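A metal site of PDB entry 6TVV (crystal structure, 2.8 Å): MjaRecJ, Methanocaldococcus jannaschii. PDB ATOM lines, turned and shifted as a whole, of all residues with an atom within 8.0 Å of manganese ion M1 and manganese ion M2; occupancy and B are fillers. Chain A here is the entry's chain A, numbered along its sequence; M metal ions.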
ATOM      1  N   HIS A  31      21.056  -2.200  -8.100  1.00  0.00           N
ATOM      2  CA  HIS A  31      21.060  -3.522  -8.768  1.00  0.00           C
ATOM      3  C   HIS A  31      21.532  -4.551  -7.726  1.00  0.00           C
ATOM      4  O   HIS A  31      22.099  -4.133  -6.683  1.00  0.00           O
ATOM      5  CB  HIS A  31      21.914  -3.341 -10.024  1.00  0.00           C
ATOM      6  CG  HIS A  31      21.647  -4.279 -11.143  1.00  0.00           C
ATOM      7  ND1 HIS A  31      22.669  -4.971 -11.764  1.00  0.00           N
ATOM      8  CD2 HIS A  31      20.508  -4.607 -11.775  1.00  0.00           C
ATOM      9  CE1 HIS A  31      22.166  -5.711 -12.717  1.00  0.00           C
ATOM     10  NE2 HIS A  31      20.831  -5.524 -12.725  1.00  0.00           N
ATOM     11  N   HIS A  32      21.282  -5.825  -7.982  1.00  0.00           N
ATOM     12  CA  HIS A  32      21.475  -6.934  -7.004  1.00  0.00           C
ATOM     13  C   HIS A  32      22.877  -7.538  -7.112  1.00  0.00           C
ATOM     14  O   HIS A  32      23.182  -8.386  -6.285  1.00  0.00           O
ATOM     15  CB  HIS A  32      20.412  -8.005  -7.207  1.00  0.00           C
ATOM     16  CG  HIS A  32      20.523  -8.724  -8.514  1.00  0.00           C
ATOM     17  ND1 HIS A  32      20.703  -8.066  -9.722  1.00  0.00           N
ATOM     18  CD2 HIS A  32      20.510 -10.039  -8.797  1.00  0.00           C
ATOM     19  CE1 HIS A  32      20.805  -8.938 -10.698  1.00  0.00           C
ATOM     20  NE2 HIS A  32      20.675 -10.159 -10.151  1.00  0.00           N
ATOM     21  N   ASP A  33      23.667  -7.128  -8.123  1.00  0.00           N
ATOM     22  CA  ASP A  33      25.079  -7.539  -8.392  1.00  0.00           C
ATOM     23  C   ASP A  33      25.999  -6.821  -7.367  1.00  0.00           C
ATOM     24  O   ASP A  33      25.579  -5.841  -6.763  1.00  0.00           O
ATOM     25  CB  ASP A  33      25.432  -7.305  -9.885  1.00  0.00           C
ATOM     26  CG  ASP A  33      25.345  -5.862 -10.416  1.00  0.00           C
ATOM     27  OD1 ASP A  33      25.037  -4.944  -9.622  1.00  0.00           O
ATOM     28  OD2 ASP A  33      25.583  -5.625 -11.615  1.00  0.00           O
ATOM     29  N   THR A  34      27.238  -7.284  -7.208  1.00  0.00           N
ATOM     30  CA  THR A  34      28.276  -6.626  -6.374  1.00  0.00           C
ATOM     31  C   THR A  34      28.384  -5.145  -6.702  1.00  0.00           C
ATOM     32  O   THR A  34      28.548  -4.357  -5.760  1.00  0.00           O
ATOM     33  CB  THR A  34      29.631  -7.325  -6.492  1.00  0.00           C
ATOM     34  OG1 THR A  34      29.418  -8.686  -6.128  1.00  0.00           O
ATOM     35  CG2 THR A  34      30.700  -6.732  -5.619  1.00  0.00           C
ATOM     36  N   ASP A  35      28.314  -4.756  -7.971  1.00  0.00           N
ATOM     37  CA  ASP A  35      28.452  -3.314  -8.364  1.00  0.00           C
ATOM     38  C   ASP A  35      27.242  -2.532  -7.828  1.00  0.00           C
ATOM     39  O   ASP A  35      27.412  -1.364  -7.418  1.00  0.00           O
ATOM     40  CB  ASP A  35      28.638  -3.179  -9.873  1.00  0.00           C
ATOM     41  CG  ASP A  35      29.005  -1.790 -10.374  1.00  0.00           C
ATOM     42  OD1 ASP A  35      29.776  -1.121  -9.620  1.00  0.00           O
ATOM     43  OD2 ASP A  35      28.559  -1.424 -11.562  1.00  0.00           O
ATOM     44  N   GLY A  36      26.080  -3.183  -7.757  1.00  0.00           N
ATOM     45  CA  GLY A  36      24.824  -2.563  -7.297  1.00  0.00           C
ATOM     46  C   GLY A  36      24.802  -2.405  -5.798  1.00  0.00           C
ATOM     47  O   GLY A  36      24.517  -1.293  -5.298  1.00  0.00           O
ATOM     48  N   SER A  39      27.360   0.082  -4.648  1.00  0.00           N
ATOM     49  CA  SER A  39      26.783   1.396  -5.007  1.00  0.00           C
ATOM     50  C   SER A  39      25.800   1.783  -3.906  1.00  0.00           C
ATOM     51  O   SER A  39      25.963   2.873  -3.367  1.00  0.00           O
ATOM     52  CB  SER A  39      26.131   1.357  -6.360  1.00  0.00           C
ATOM     53  OG  SER A  39      27.120   1.317  -7.379  1.00  0.00           O
ATOM     54  N   GLU A  60      16.015  -6.181 -10.005  1.00  0.00           N
ATOM     55  CA  GLU A  60      16.715  -7.148 -10.892  1.00  0.00           C
ATOM     56  C   GLU A  60      16.946  -6.441 -12.234  1.00  0.00           C
ATOM     57  O   GLU A  60      18.103  -6.288 -12.621  1.00  0.00           O
ATOM     58  CB  GLU A  60      15.919  -8.444 -11.052  1.00  0.00           C
ATOM     59  CG  GLU A  60      15.394  -9.001  -9.738  1.00  0.00           C
ATOM     60  CD  GLU A  60      16.173 -10.193  -9.215  1.00  0.00           C
ATOM     61  OE1 GLU A  60      15.895 -11.318  -9.667  1.00  0.00           O
ATOM     62  OE2 GLU A  60      17.053  -9.980  -8.357  1.00  0.00           O
ATOM     63  N   ALA A  84      21.326   3.847  -9.546  1.00  0.00           N
ATOM     64  CA  ALA A  84      22.721   3.376  -9.475  1.00  0.00           C
ATOM     65  C   ALA A  84      23.030   2.668 -10.777  1.00  0.00           C
ATOM     66  O   ALA A  84      23.072   3.352 -11.814  1.00  0.00           O
ATOM     67  CB  ALA A  84      22.915   2.491  -8.290  1.00  0.00           C
ATOM     68  N   ASP A  85      23.240   1.368 -10.777  1.00  0.00           N
ATOM     69  CA  ASP A  85      23.973   0.708 -11.902  1.00  0.00           C
ATOM     70  C   ASP A  85      22.931   0.473 -13.023  1.00  0.00           C
ATOM     71  O   ASP A  85      22.704  -0.680 -13.429  1.00  0.00           O
ATOM     72  CB  ASP A  85      24.792  -0.422 -11.268  1.00  0.00           C
ATOM     73  CG  ASP A  85      25.204  -1.617 -12.098  1.00  0.00           C
ATOM     74  OD1 ASP A  85      25.873  -1.394 -13.151  1.00  0.00           O
ATOM     75  OD2 ASP A  85      24.926  -2.763 -11.623  1.00  0.00           O
ATOM     76  N   MET A  86      22.293   1.557 -13.487  1.00  0.00           N
ATOM     77  CA  MET A  86      21.052   1.542 -14.317  1.00  0.00           C
ATOM     78  C   MET A  86      20.539   2.974 -14.516  1.00  0.00           C
ATOM     79  O   MET A  86      20.986   3.839 -13.798  1.00  0.00           O
ATOM     80  CB  MET A  86      19.916   0.749 -13.682  1.00  0.00           C
ATOM     81  CG  MET A  86      19.279   1.462 -12.498  1.00  0.00           C
ATOM     82  SD  MET A  86      18.234   0.403 -11.455  1.00  0.00           S
ATOM     83  CE  MET A  86      19.200  -1.100 -11.346  1.00  0.00           C
ATOM     84  N   ASP A 105      25.486   5.775 -13.818  1.00  0.00           N
ATOM     85  CA  ASP A 105      25.504   4.557 -14.668  1.00  0.00           C
ATOM     86  C   ASP A 105      26.831   4.546 -15.438  1.00  0.00           C
ATOM     87  O   ASP A 105      27.586   5.547 -15.373  1.00  0.00           O
ATOM     88  CB  ASP A 105      24.253   4.502 -15.557  1.00  0.00           C
ATOM     89  CG  ASP A 105      23.837   3.115 -16.008  1.00  0.00           C
ATOM     90  OD1 ASP A 105      24.629   2.183 -15.763  1.00  0.00           O
ATOM     91  OD2 ASP A 105      22.726   2.988 -16.633  1.00  0.00           O
ATOM     92  N   HIS A 106      27.129   3.418 -16.054  1.00  0.00           N
ATOM     93  CA  HIS A 106      28.349   3.177 -16.880  1.00  0.00           C
ATOM     94  C   HIS A 106      27.988   2.255 -18.049  1.00  0.00           C
ATOM     95  O   HIS A 106      28.887   1.998 -18.866  1.00  0.00           O
ATOM     96  CB  HIS A 106      29.481   2.594 -16.017  1.00  0.00           C
ATOM     97  CG  HIS A 106      29.255   1.193 -15.552  1.00  0.00           C
ATOM     98  ND1 HIS A 106      30.136   0.193 -15.833  1.00  0.00           N
ATOM     99  CD2 HIS A 106      28.276   0.629 -14.803  1.00  0.00           C
ATOM    100  CE1 HIS A 106      29.712  -0.939 -15.292  1.00  0.00           C
ATOM    101  NE2 HIS A 106      28.582  -0.714 -14.650  1.00  0.00           N
ATOM    102  N   HIS A 107      26.746   1.787 -18.107  1.00  0.00           N
ATOM    103  CA  HIS A 107      26.149   1.111 -19.289  1.00  0.00           C
ATOM    104  C   HIS A 107      26.140   2.119 -20.447  1.00  0.00           C
ATOM    105  O   HIS A 107      26.192   3.315 -20.242  1.00  0.00           O
ATOM    106  CB  HIS A 107      24.764   0.532 -18.930  1.00  0.00           C
ATOM    107  CG  HIS A 107      24.790  -0.580 -17.923  1.00  0.00           C
ATOM    108  ND1 HIS A 107      24.127  -1.778 -18.128  1.00  0.00           N
ATOM    109  CD2 HIS A 107      25.344  -0.658 -16.688  1.00  0.00           C
ATOM    110  CE1 HIS A 107      24.293  -2.547 -17.080  1.00  0.00           C
ATOM    111  NE2 HIS A 107      25.042  -1.886 -16.171  1.00  0.00           N
ATOM    112  N   GLY A 132      32.582   2.061 -19.659  1.00  0.00           N
ATOM    113  CA  GLY A 132      32.031   1.303 -18.514  1.00  0.00           C
ATOM    114  C   GLY A 132      32.179  -0.170 -18.745  1.00  0.00           C
ATOM    115  O   GLY A 132      31.480  -0.944 -18.069  1.00  0.00           O
ATOM    116  N   ILE A 136      35.659   1.963 -15.566  1.00  0.00           N
ATOM    117  CA  ILE A 136      34.759   2.543 -14.511  1.00  0.00           C
ATOM    118  C   ILE A 136      33.548   1.613 -14.324  1.00  0.00           C
ATOM    119  O   ILE A 136      33.120   0.986 -15.296  1.00  0.00           O
ATOM    120  CB  ILE A 136      34.350   3.986 -14.876  1.00  0.00           C
ATOM    121  CG1 ILE A 136      33.699   4.762 -13.733  1.00  0.00           C
ATOM    122  CG2 ILE A 136      33.415   3.981 -16.080  1.00  0.00           C
ATOM    123  CD1 ILE A 136      34.659   5.234 -12.691  1.00  0.00           C
ATOM    124  N   THR A 137      33.021   1.573 -13.099  1.00  0.00           N
ATOM    125  CA  THR A 137      31.837   0.818 -12.639  1.00  0.00           C
ATOM    126  C   THR A 137      30.901   1.804 -11.937  1.00  0.00           C
ATOM    127  O   THR A 137      31.302   2.972 -11.748  1.00  0.00           O
ATOM    128  CB  THR A 137      32.249  -0.313 -11.681  1.00  0.00           C
ATOM    129  OG1 THR A 137      33.102   0.216 -10.663  1.00  0.00           O
ATOM    130  CG2 THR A 137      33.026  -1.424 -12.362  1.00  0.00           C
ATOM    131  N   ALA A 138      29.717   1.359 -11.535  1.00  0.00           N
ATOM    132  CA  ALA A 138      28.735   2.219 -10.842  1.00  0.00           C
ATOM    133  C   ALA A 138      29.282   2.654  -9.477  1.00  0.00           C
ATOM    134  O   ALA A 138      29.216   3.857  -9.131  1.00  0.00           O
ATOM    135  CB  ALA A 138      27.434   1.490 -10.713  1.00  0.00           C
ATOM    136  N   SER A 139      29.804   1.690  -8.727  1.00  0.00           N
ATOM    137  CA  SER A 139      30.510   1.910  -7.441  1.00  0.00           C
ATOM    138  C   SER A 139      31.493   3.059  -7.605  1.00  0.00           C
ATOM    139  O   SER A 139      31.506   3.971  -6.766  1.00  0.00           O
ATOM    140  CB  SER A 139      31.204   0.671  -7.022  1.00  0.00           C
ATOM    141  OG  SER A 139      32.012   0.231  -8.090  1.00  0.00           O
ATOM    142  N   GLY A 161      33.319  -2.945  -6.227  1.00  0.00           N
ATOM    143  CA  GLY A 161      32.558  -2.907  -7.495  1.00  0.00           C
ATOM    144  C   GLY A 161      33.451  -3.178  -8.681  1.00  0.00           C
ATOM    145  O   GLY A 161      33.044  -3.947  -9.602  1.00  0.00           O
ATOM    146  N   GLY A 164      33.875  -6.701  -8.601  1.00  0.00           N
ATOM    147  CA  GLY A 164      32.554  -7.262  -8.928  1.00  0.00           C
ATOM    148  C   GLY A 164      32.364  -7.375 -10.424  1.00  0.00           C
ATOM    149  O   GLY A 164      32.025  -8.465 -10.881  1.00  0.00           O
ATOM    150  N   ASP A 165      32.589  -6.277 -11.160  1.00  0.00           N
ATOM    151  CA  ASP A 165      32.303  -6.149 -12.616  1.00  0.00           C
ATOM    152  C   ASP A 165      33.517  -6.618 -13.430  1.00  0.00           C
ATOM    153  O   ASP A 165      33.507  -6.397 -14.644  1.00  0.00           O
ATOM    154  CB  ASP A 165      31.924  -4.709 -12.978  1.00  0.00           C
ATOM    155  CG  ASP A 165      30.451  -4.367 -12.828  1.00  0.00           C
ATOM    156  OD1 ASP A 165      29.666  -5.289 -12.519  1.00  0.00           O
ATOM    157  OD2 ASP A 165      30.097  -3.173 -13.017  1.00  0.00           O
ATOM    158  N   GLN A 167      36.841  -5.640 -13.619  1.00  0.00           N
ATOM    159  CA  GLN A 167      37.614  -4.540 -14.280  1.00  0.00           C
ATOM    160  C   GLN A 167      38.949  -4.308 -13.557  1.00  0.00           C
ATOM    161  O   GLN A 167      39.471  -3.166 -13.640  1.00  0.00           O
ATOM    162  CB  GLN A 167      36.781  -3.252 -14.340  1.00  0.00           C
ATOM    163  CG  GLN A 167      35.482  -3.429 -15.112  1.00  0.00           C
ATOM    164  CD  GLN A 167      34.805  -2.126 -15.490  1.00  0.00           C
ATOM    165  OE1 GLN A 167      35.311  -1.034 -15.201  1.00  0.00           O
ATOM    166  NE2 GLN A 167      33.636  -2.252 -16.106  1.00  0.00           N
HETATM  167 MN    MN M   1      27.731  -2.847 -13.397  1.00  0.00          MN
HETATM  168 MN    MN M   2      24.996  -4.581 -13.202  1.00  0.00          MN
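OD1 of Asp 85 is bound to manganese ion M1, 2.4 Å away.
OD2 of Asp 165 is bound to manganese ion M1 (2.4 Å).
The side-chain carboxylate (OD2) of Asp 35 binds manganese ion M1 (2.5 Å).
A ring nitrogen (NE2) of His 106 binds manganese ion M1, at 2.6 Å.
ND1 of His 31 lies close to OD1 of Asp 33.
OD2 of Asp 85 lies close to ND1 of His 31 (3.2 Å).
The side-chain carboxylate (OD1) of Asp 85 sits close to a ring nitrogen (NE2) of His 107 (3.2 Å).
The side-chain carboxylate (OD1) of Asp 35 lies within hydrogen-bond range of the backbone NH (N) of Ser 139.
The side-chain hydroxyl (OG) of Ser 39 is in hydrogen-bond range of the backbone carbonyl oxygen (O) of Asp 35, at 2.7 Å.
ND1 of His 106 sits at hydrogen-bond distance from O of Gly 132.
ND1 of His 106 is in hydrogen-bond range of O of Ile 136, at 3.1 Å.
OD1 of Asp 105 lies close to N of His 107, 3.2 Å away.
Within 4 Å of manganese ion M2: His 31, Asp 33 and Asp 85.
Merely in contact with manganese ion M1: His 107 (3.98 Å).
Six residues have an atom within 4 Å of manganese ion M1: Asp 33, Asp 35, Asp 85, His 106, His 107 and Asp 165.
The nearest printed residue that does not touch manganese ion M1 is Ala 138 (5.0 Å).
Manganese ion M2 is bound by OD2 of Asp 33 (2.0 Å) and OD2 of Asp 85 (2.4 Å).
Slightly farther from manganese ion M2 lies ND1 of His 31 (2.8 Å).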
